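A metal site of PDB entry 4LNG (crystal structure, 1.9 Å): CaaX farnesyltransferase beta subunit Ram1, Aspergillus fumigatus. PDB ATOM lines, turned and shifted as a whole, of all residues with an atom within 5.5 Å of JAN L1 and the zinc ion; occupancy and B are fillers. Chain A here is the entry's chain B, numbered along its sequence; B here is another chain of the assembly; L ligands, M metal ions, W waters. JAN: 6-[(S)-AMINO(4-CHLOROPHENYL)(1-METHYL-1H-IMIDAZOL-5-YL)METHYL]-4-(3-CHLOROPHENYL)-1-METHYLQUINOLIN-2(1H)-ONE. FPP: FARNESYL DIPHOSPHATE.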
ATOM      1  N   LEU A 147      -0.669  -5.688 -10.396  1.00  0.00           N
ATOM      2  CA  LEU A 147      -1.679  -5.057 -11.246  1.00  0.00           C
ATOM      3  C   LEU A 147      -1.093  -4.478 -12.534  1.00  0.00           C
ATOM      4  O   LEU A 147      -1.820  -3.878 -13.332  1.00  0.00           O
ATOM      5  CB  LEU A 147      -2.411  -3.959 -10.473  1.00  0.00           C
ATOM      6  CG  LEU A 147      -3.297  -4.436  -9.317  1.00  0.00           C
ATOM      7  CD1 LEU A 147      -3.925  -3.251  -8.584  1.00  0.00           C
ATOM      8  CD2 LEU A 147      -4.382  -5.376  -9.834  1.00  0.00           C
ATOM      9  N   SER A 150      -2.798  -5.137 -15.666  1.00  0.00           N
ATOM     10  CA  SER A 150      -4.223  -4.804 -15.608  1.00  0.00           C
ATOM     11  C   SER A 150      -4.469  -3.303 -15.423  1.00  0.00           C
ATOM     12  O   SER A 150      -5.556  -2.906 -14.989  1.00  0.00           O
ATOM     13  CB  SER A 150      -4.901  -5.586 -14.487  1.00  0.00           C
ATOM     14  OG  SER A 150      -4.755  -6.981 -14.679  1.00  0.00           O
ATOM     15  N   TRP A 153      -7.648  -1.829 -16.914  1.00  0.00           N
ATOM     16  CA  TRP A 153      -8.815  -2.160 -16.081  1.00  0.00           C
ATOM     17  C   TRP A 153      -8.983  -1.133 -14.967  1.00  0.00           C
ATOM     18  O   TRP A 153     -10.097  -0.698 -14.681  1.00  0.00           O
ATOM     19  CB  TRP A 153      -8.655  -3.544 -15.441  1.00  0.00           C
ATOM     20  CG  TRP A 153      -9.188  -4.720 -16.207  1.00  0.00           C
ATOM     21  CD1 TRP A 153      -8.520  -5.864 -16.518  1.00  0.00           C
ATOM     22  CD2 TRP A 153     -10.528  -4.892 -16.728  1.00  0.00           C
ATOM     23  NE1 TRP A 153      -9.339  -6.725 -17.208  1.00  0.00           N
ATOM     24  CE2 TRP A 153     -10.567  -6.153 -17.351  1.00  0.00           C
ATOM     25  CE3 TRP A 153     -11.682  -4.098 -16.729  1.00  0.00           C
ATOM     26  CZ2 TRP A 153     -11.720  -6.645 -17.974  1.00  0.00           C
ATOM     27  CZ3 TRP A 153     -12.822  -4.585 -17.335  1.00  0.00           C
ATOM     28  CH2 TRP A 153     -12.836  -5.844 -17.954  1.00  0.00           C
ATOM     29  N   TRP A 157     -12.465   0.929 -14.246  1.00  0.00           N
ATOM     30  CA  TRP A 157     -13.238   0.759 -13.012  1.00  0.00           C
ATOM     31  C   TRP A 157     -13.469   2.102 -12.322  1.00  0.00           C
ATOM     32  O   TRP A 157     -14.577   2.391 -11.848  1.00  0.00           O
ATOM     33  CB  TRP A 157     -12.536  -0.208 -12.055  1.00  0.00           C
ATOM     34  CG  TRP A 157     -12.430  -1.621 -12.566  1.00  0.00           C
ATOM     35  CD1 TRP A 157     -13.343  -2.283 -13.340  1.00  0.00           C
ATOM     36  CD2 TRP A 157     -11.352  -2.530 -12.347  1.00  0.00           C
ATOM     37  NE1 TRP A 157     -12.884  -3.560 -13.615  1.00  0.00           N
ATOM     38  CE2 TRP A 157     -11.664  -3.732 -13.015  1.00  0.00           C
ATOM     39  CE3 TRP A 157     -10.136  -2.450 -11.648  1.00  0.00           C
ATOM     40  CZ2 TRP A 157     -10.821  -4.840 -12.999  1.00  0.00           C
ATOM     41  CZ3 TRP A 157      -9.300  -3.550 -11.641  1.00  0.00           C
ATOM     42  CH2 TRP A 157      -9.646  -4.736 -12.311  1.00  0.00           C
ATOM     43  N   ARG A 252     -15.137 -15.066 -21.557  1.00  0.00           N
ATOM     44  CA  ARG A 252     -14.717 -13.702 -21.240  1.00  0.00           C
ATOM     45  C   ARG A 252     -14.019 -13.116 -22.454  1.00  0.00           C
ATOM     46  O   ARG A 252     -14.236 -11.949 -22.807  1.00  0.00           O
ATOM     47  CB  ARG A 252     -13.784 -13.695 -20.023  1.00  0.00           C
ATOM     48  CG  ARG A 252     -12.810 -12.537 -20.010  1.00  0.00           C
ATOM     49  CD  ARG A 252     -11.701 -12.753 -18.988  1.00  0.00           C
ATOM     50  NE  ARG A 252     -10.895 -13.924 -19.292  1.00  0.00           N
ATOM     51  CZ  ARG A 252      -9.564 -13.975 -19.167  1.00  0.00           C
ATOM     52  NH1 ARG A 252      -8.899 -12.914 -18.741  1.00  0.00           N
ATOM     53  NH2 ARG A 252      -8.915 -15.084 -19.473  1.00  0.00           N
ATOM     54  N   ASP A 365     -20.948 -12.145  -3.099  1.00  0.00           N
ATOM     55  CA  ASP A 365     -19.852 -11.246  -3.430  1.00  0.00           C
ATOM     56  C   ASP A 365     -20.452 -10.042  -4.150  1.00  0.00           C
ATOM     57  O   ASP A 365     -21.176 -10.192  -5.128  1.00  0.00           O
ATOM     58  CB  ASP A 365     -18.842 -11.978  -4.313  1.00  0.00           C
ATOM     59  CG  ASP A 365     -17.660 -11.110  -4.748  1.00  0.00           C
ATOM     60  OD1 ASP A 365     -17.749  -9.861  -4.712  1.00  0.00           O
ATOM     61  OD2 ASP A 365     -16.633 -11.695  -5.153  1.00  0.00           O
ATOM     62  N   GLY A 366     -20.139  -8.841  -3.659  1.00  0.00           N
ATOM     63  CA  GLY A 366     -20.682  -7.615  -4.208  1.00  0.00           C
ATOM     64  C   GLY A 366     -20.479  -7.388  -5.700  1.00  0.00           C
ATOM     65  O   GLY A 366     -21.274  -6.697  -6.328  1.00  0.00           O
ATOM     66  N   CYS A 367     -19.419  -7.945  -6.279  1.00  0.00           N
ATOM     67  CA  CYS A 367     -19.188  -7.734  -7.705  1.00  0.00           C
ATOM     68  C   CYS A 367     -20.206  -8.479  -8.564  1.00  0.00           C
ATOM     69  O   CYS A 367     -20.467  -8.095  -9.703  1.00  0.00           O
ATOM     70  CB  CYS A 367     -17.750  -8.073  -8.128  1.00  0.00           C
ATOM     71  SG  CYS A 367     -17.319  -9.834  -8.158  1.00  0.00           S
ATOM     72  N   TYR A 368     -20.789  -9.542  -8.019  1.00  0.00           N
ATOM     73  CA  TYR A 368     -21.820 -10.287  -8.751  1.00  0.00           C
ATOM     74  C   TYR A 368     -23.133  -9.495  -8.814  1.00  0.00           C
ATOM     75  O   TYR A 368     -24.066  -9.902  -9.496  1.00  0.00           O
ATOM     76  CB  TYR A 368     -22.008 -11.688  -8.155  1.00  0.00           C
ATOM     77  CG  TYR A 368     -20.745 -12.507  -8.202  1.00  0.00           C
ATOM     78  CD1 TYR A 368     -19.921 -12.472  -9.322  1.00  0.00           C
ATOM     79  CD2 TYR A 368     -20.342 -13.277  -7.121  1.00  0.00           C
ATOM     80  CE1 TYR A 368     -18.738 -13.197  -9.371  1.00  0.00           C
ATOM     81  CE2 TYR A 368     -19.160 -14.015  -7.159  1.00  0.00           C
ATOM     82  CZ  TYR A 368     -18.372 -13.965  -8.291  1.00  0.00           C
ATOM     83  OH  TYR A 368     -17.197 -14.681  -8.349  1.00  0.00           O
ATOM     84  N   TRP A 371     -22.284  -8.950 -12.399  1.00  0.00           N
ATOM     85  CA  TRP A 371     -22.181 -10.164 -13.235  1.00  0.00           C
ATOM     86  C   TRP A 371     -23.473 -10.970 -13.248  1.00  0.00           C
ATOM     87  O   TRP A 371     -23.947 -11.373 -14.304  1.00  0.00           O
ATOM     88  CB  TRP A 371     -20.982 -11.037 -12.841  1.00  0.00           C
ATOM     89  CG  TRP A 371     -19.669 -10.293 -12.884  1.00  0.00           C
ATOM     90  CD1 TRP A 371     -18.866  -9.994 -11.816  1.00  0.00           C
ATOM     91  CD2 TRP A 371     -19.038  -9.728 -14.039  1.00  0.00           C
ATOM     92  NE1 TRP A 371     -17.766  -9.288 -12.247  1.00  0.00           N
ATOM     93  CE2 TRP A 371     -17.848  -9.101 -13.604  1.00  0.00           C
ATOM     94  CE3 TRP A 371     -19.361  -9.677 -15.392  1.00  0.00           C
ATOM     95  CZ2 TRP A 371     -16.978  -8.448 -14.471  1.00  0.00           C
ATOM     96  CZ3 TRP A 371     -18.501  -9.029 -16.267  1.00  0.00           C
ATOM     97  CH2 TRP A 371     -17.325  -8.424 -15.797  1.00  0.00           C
ATOM     98  N   ASP A 423     -16.018  -6.728  -1.694  1.00  0.00           N
ATOM     99  CA  ASP A 423     -16.553  -8.057  -1.961  1.00  0.00           C
ATOM    100  C   ASP A 423     -17.598  -8.406  -0.891  1.00  0.00           C
ATOM    101  O   ASP A 423     -18.748  -8.681  -1.199  1.00  0.00           O
ATOM    102  CB  ASP A 423     -15.368  -9.041  -1.953  1.00  0.00           C
ATOM    103  CG  ASP A 423     -15.758 -10.517  -1.965  1.00  0.00           C
ATOM    104  OD1 ASP A 423     -16.939 -10.885  -1.747  1.00  0.00           O
ATOM    105  OD2 ASP A 423     -14.846 -11.341  -2.170  1.00  0.00           O
ATOM    106  N   ASP A 430     -11.702  -2.383  -3.030  1.00  0.00           N
ATOM    107  CA  ASP A 430     -10.826  -2.166  -4.178  1.00  0.00           C
ATOM    108  C   ASP A 430     -11.668  -1.535  -5.288  1.00  0.00           C
ATOM    109  O   ASP A 430     -12.893  -1.521  -5.192  1.00  0.00           O
ATOM    110  CB  ASP A 430     -10.163  -3.468  -4.639  1.00  0.00           C
ATOM    111  CG  ASP A 430     -11.168  -4.541  -5.018  1.00  0.00           C
ATOM    112  OD1 ASP A 430     -11.720  -4.461  -6.139  1.00  0.00           O
ATOM    113  OD2 ASP A 430     -11.394  -5.459  -4.207  1.00  0.00           O
ATOM    114  N   SER A 431     -11.020  -1.000  -6.313  1.00  0.00           N
ATOM    115  CA  SER A 431     -11.756  -0.264  -7.328  1.00  0.00           C
ATOM    116  C   SER A 431     -12.604  -1.187  -8.216  1.00  0.00           C
ATOM    117  O   SER A 431     -13.612  -0.764  -8.762  1.00  0.00           O
ATOM    118  CB  SER A 431     -10.844   0.639  -8.160  1.00  0.00           C
ATOM    119  OG  SER A 431      -9.912  -0.106  -8.919  1.00  0.00           O
ATOM    120  N   TYR A 432     -12.178  -2.443  -8.348  1.00  0.00           N
ATOM    121  CA  TYR A 432     -12.952  -3.445  -9.088  1.00  0.00           C
ATOM    122  C   TYR A 432     -14.293  -3.694  -8.409  1.00  0.00           C
ATOM    123  O   TYR A 432     -15.354  -3.625  -9.047  1.00  0.00           O
ATOM    124  CB  TYR A 432     -12.143  -4.750  -9.235  1.00  0.00           C
ATOM    125  CG  TYR A 432     -12.980  -5.973  -9.592  1.00  0.00           C
ATOM    126  CD1 TYR A 432     -13.192  -6.335 -10.913  1.00  0.00           C
ATOM    127  CD2 TYR A 432     -13.523  -6.780  -8.599  1.00  0.00           C
ATOM    128  CE1 TYR A 432     -13.949  -7.460 -11.242  1.00  0.00           C
ATOM    129  CE2 TYR A 432     -14.279  -7.895  -8.907  1.00  0.00           C
ATOM    130  CZ  TYR A 432     -14.493  -8.235 -10.228  1.00  0.00           C
ATOM    131  OH  TYR A 432     -15.242  -9.359 -10.527  1.00  0.00           O
ATOM    132  N   HIS A 433     -14.265  -3.975  -7.109  1.00  0.00           N
ATOM    133  CA  HIS A 433     -15.493  -4.225  -6.365  1.00  0.00           C
ATOM    134  C   HIS A 433     -16.329  -2.963  -6.190  1.00  0.00           C
ATOM    135  O   HIS A 433     -17.549  -3.025  -6.114  1.00  0.00           O
ATOM    136  CB  HIS A 433     -15.203  -4.907  -5.020  1.00  0.00           C
ATOM    137  CG  HIS A 433     -14.861  -6.361  -5.147  1.00  0.00           C
ATOM    138  ND1 HIS A 433     -13.569  -6.835  -5.034  1.00  0.00           N
ATOM    139  CD2 HIS A 433     -15.635  -7.432  -5.421  1.00  0.00           C
ATOM    140  CE1 HIS A 433     -13.568  -8.141  -5.211  1.00  0.00           C
ATOM    141  NE2 HIS A 433     -14.809  -8.532  -5.453  1.00  0.00           N
ATOM    142  N   TYR B 123      -4.057 -17.985 -12.237  1.00  0.00           N
ATOM    143  CA  TYR B 123      -4.576 -18.840 -13.303  1.00  0.00           C
ATOM    144  C   TYR B 123      -3.691 -18.905 -14.551  1.00  0.00           C
ATOM    145  O   TYR B 123      -3.816 -19.837 -15.345  1.00  0.00           O
ATOM    146  CB  TYR B 123      -6.019 -18.465 -13.665  1.00  0.00           C
ATOM    147  CG  TYR B 123      -6.180 -17.095 -14.295  1.00  0.00           C
ATOM    148  CD1 TYR B 123      -6.052 -16.925 -15.663  1.00  0.00           C
ATOM    149  CD2 TYR B 123      -6.476 -15.983 -13.511  1.00  0.00           C
ATOM    150  CE1 TYR B 123      -6.211 -15.675 -16.239  1.00  0.00           C
ATOM    151  CE2 TYR B 123      -6.626 -14.728 -14.089  1.00  0.00           C
ATOM    152  CZ  TYR B 123      -6.494 -14.581 -15.448  1.00  0.00           C
ATOM    153  OH  TYR B 123      -6.637 -13.344 -16.038  1.00  0.00           O
HETATM  154  C1  JAN L   1     -13.230 -14.358  -8.783  1.00  0.00           C
HETATM  155  N1  JAN L   1     -13.292 -12.902  -8.325  1.00  0.00           N
HETATM  156  C2  JAN L   1     -14.404 -12.524  -7.759  1.00  0.00           C
HETATM  157  N2  JAN L   1     -14.249 -11.377  -7.267  1.00  0.00           N
HETATM  158  C3  JAN L   1     -13.010 -10.742  -7.516  1.00  0.00           C
HETATM  159  C4  JAN L   1     -12.282 -11.915  -8.069  1.00  0.00           C
HETATM  160  C5  JAN L   1     -10.731 -11.949  -8.682  1.00  0.00           C
HETATM  161  C6  JAN L   1     -10.939 -12.321 -10.189  1.00  0.00           C
HETATM  162  C7  JAN L   1     -11.837 -11.597 -10.905  1.00  0.00           C
HETATM  163  C8  JAN L   1     -11.970 -11.606 -12.306  1.00  0.00           C
HETATM  164  C9  JAN L   1     -10.735 -12.459 -12.665  1.00  0.00           C
HETATM  165 CL1  JAN L   1     -10.744 -12.378 -14.605  1.00  0.00          CL
HETATM  166  C10 JAN L   1      -9.905 -13.125 -12.078  1.00  0.00           C
HETATM  167  C11 JAN L   1      -9.990 -13.072 -10.632  1.00  0.00           C
HETATM  168  N3  JAN L   1     -10.237 -13.151  -8.089  1.00  0.00           N
HETATM  169  C12 JAN L   1     -10.241 -10.558  -8.270  1.00  0.00           C
HETATM  170  C13 JAN L   1      -9.812  -9.834  -9.202  1.00  0.00           C
HETATM  171  C14 JAN L   1      -9.117  -8.722  -8.775  1.00  0.00           C
HETATM  172  C15 JAN L   1     -10.040 -10.541  -6.908  1.00  0.00           C
HETATM  173  C16 JAN L   1      -9.422  -9.151  -6.374  1.00  0.00           C
HETATM  174  C17 JAN L   1      -9.127  -8.290  -7.635  1.00  0.00           C
HETATM  175  N4  JAN L   1      -8.442  -7.119  -7.073  1.00  0.00           N
HETATM  176  C18 JAN L   1      -8.414  -6.829  -5.528  1.00  0.00           C
HETATM  177  C19 JAN L   1      -8.188  -6.119  -7.955  1.00  0.00           C
HETATM  178  O1  JAN L   1      -7.720  -5.061  -7.469  1.00  0.00           O
HETATM  179  C20 JAN L   1      -8.336  -6.526  -9.271  1.00  0.00           C
HETATM  180  C21 JAN L   1      -8.639  -7.745  -9.765  1.00  0.00           C
HETATM  181  C22 JAN L   1      -8.784  -8.009 -11.199  1.00  0.00           C
HETATM  182  C23 JAN L   1     -10.124  -8.114 -11.793  1.00  0.00           C
HETATM  183  C24 JAN L   1      -9.974  -8.338 -13.148  1.00  0.00           C
HETATM  184 CL2  JAN L   1     -11.527  -8.520 -13.996  1.00  0.00          CL
HETATM  185  C25 JAN L   1      -8.772  -8.619 -14.007  1.00  0.00           C
HETATM  186  C26 JAN L   1      -7.581  -8.258 -13.267  1.00  0.00           C
HETATM  187  C27 JAN L   1      -7.671  -8.085 -11.978  1.00  0.00           C
HETATM  188  C1  FPP L   2     -13.579 -17.951  -9.594  1.00  0.00           C
HETATM  189  O1  FPP L   2     -12.764 -17.469  -8.564  1.00  0.00           O
HETATM  190  C2  FPP L   2     -14.150 -17.047 -10.470  1.00  0.00           C
HETATM  191  C3  FPP L   2     -14.296 -17.343 -11.933  1.00  0.00           C
HETATM  192  C4  FPP L   2     -13.025 -17.936 -12.472  1.00  0.00           C
HETATM  193  C5  FPP L   2     -14.751 -16.055 -12.682  1.00  0.00           C
HETATM  194  C6  FPP L   2     -13.746 -14.887 -12.800  1.00  0.00           C
HETATM  195  C7  FPP L   2     -13.951 -13.839 -13.731  1.00  0.00           C
HETATM  196  C8  FPP L   2     -15.081 -12.837 -13.537  1.00  0.00           C
HETATM  197  C10 FPP L   2     -15.135 -12.311 -12.130  1.00  0.00           C
HETATM  198  C9  FPP L   2     -15.061 -11.731 -14.568  1.00  0.00           C
HETATM  199  C11 FPP L   2     -14.909 -12.139 -16.012  1.00  0.00           C
HETATM  200  C12 FPP L   2     -15.328 -11.293 -17.029  1.00  0.00           C
HETATM  201  C13 FPP L   2     -14.595 -10.000 -17.348  1.00  0.00           C
HETATM  202  C14 FPP L   2     -13.083 -10.048 -17.166  1.00  0.00           C
HETATM  203  C15 FPP L   2     -15.049  -9.297 -18.590  1.00  0.00           C
HETATM  204  PA  FPP L   2     -13.210 -17.558  -7.044  1.00  0.00           P
HETATM  205  O1A FPP L   2     -13.225 -19.003  -6.615  1.00  0.00           O
HETATM  206  O2A FPP L   2     -12.212 -16.796  -6.222  1.00  0.00           O
HETATM  207  O3A FPP L   2     -14.602 -16.859  -6.899  1.00  0.00           O
HETATM  208  PB  FPP L   2     -15.959 -17.567  -6.495  1.00  0.00           P
HETATM  209  O1B FPP L   2     -15.842 -18.286  -5.166  1.00  0.00           O
HETATM  210  O2B FPP L   2     -16.410 -18.534  -7.556  1.00  0.00           O
HETATM  211  O3B FPP L   2     -16.985 -16.456  -6.340  1.00  0.00           O
HETATM  212 ZN    ZN M   1     -15.839 -10.143  -6.361  1.00  0.00          ZN
HETATM  213  O   HOH W   1     -10.708 -12.848  -4.506  1.00  0.00           O
HETATM  214  O   HOH W   2     -10.186 -16.231  -8.808  1.00  0.00           O
HETATM  215  O   HOH W   3      -7.486 -13.249  -7.934  1.00  0.00           O
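ND1 of His 433 lies within hydrogen-bond range of OD2 of Asp 430, at 2.7 Å.
SG of Cys 367 sits close to OH of Tyr 432 (3.2 Å).
The backbone NH (N) of Tyr 432 lies within hydrogen-bond range of the side-chain carboxylate (OD1) of Asp 430 (3.0 Å).
OH of Tyr 432 is in hydrogen-bond range of NE1 of Trp 371, 3.1 Å away.
Water W2 bridges an oxygen (O1) of FPP L2 and a nitrogen (N3) of JAN L1.
Tyr 432 touches the zinc ion.
Four residues have an atom within 4 Å of the zinc ion: Asp 365, Cys 367, Tyr 432 and His 433.
The nearest printed residue that does not touch the zinc ion is Asp 423 (4.4 Å).
Ser 150 touches JAN L1 (OG to C26, 3.4 Å).
Trp 153 touches JAN L1 (CD1 to C25, 3.7 Å).
CH2 of Trp 157 touches C23 of JAN L1, 3.5 Å away.
OH of Tyr 368 touches C2 of JAN L1, 3.6 Å away.
Asp 430 touches JAN L1 (OD2 to C18, 3.5 Å).
Tyr 432 touches JAN L1 (CE2 to C3, 3.4 Å).
Hydrophobic or aromatic side chains within 4 Å of JAN L1: Trp 153, Trp 157, Tyr 432 and His 433.
Within 4 Å of JAN L1: Ser 150, Trp 153, Trp 157, Asp 365, Cys 367, Tyr 368, Asp 430, Tyr 432 and His 433.
OH of Tyr 368 sits at hydrogen-bond distance from O3B of FPP L2, at 2.7 Å.
The zinc ion is bound by NE2 of His 433, OD2 of Asp 365, N2 of JAN L1, SG of Cys 367 and OD1 of Asp 365.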
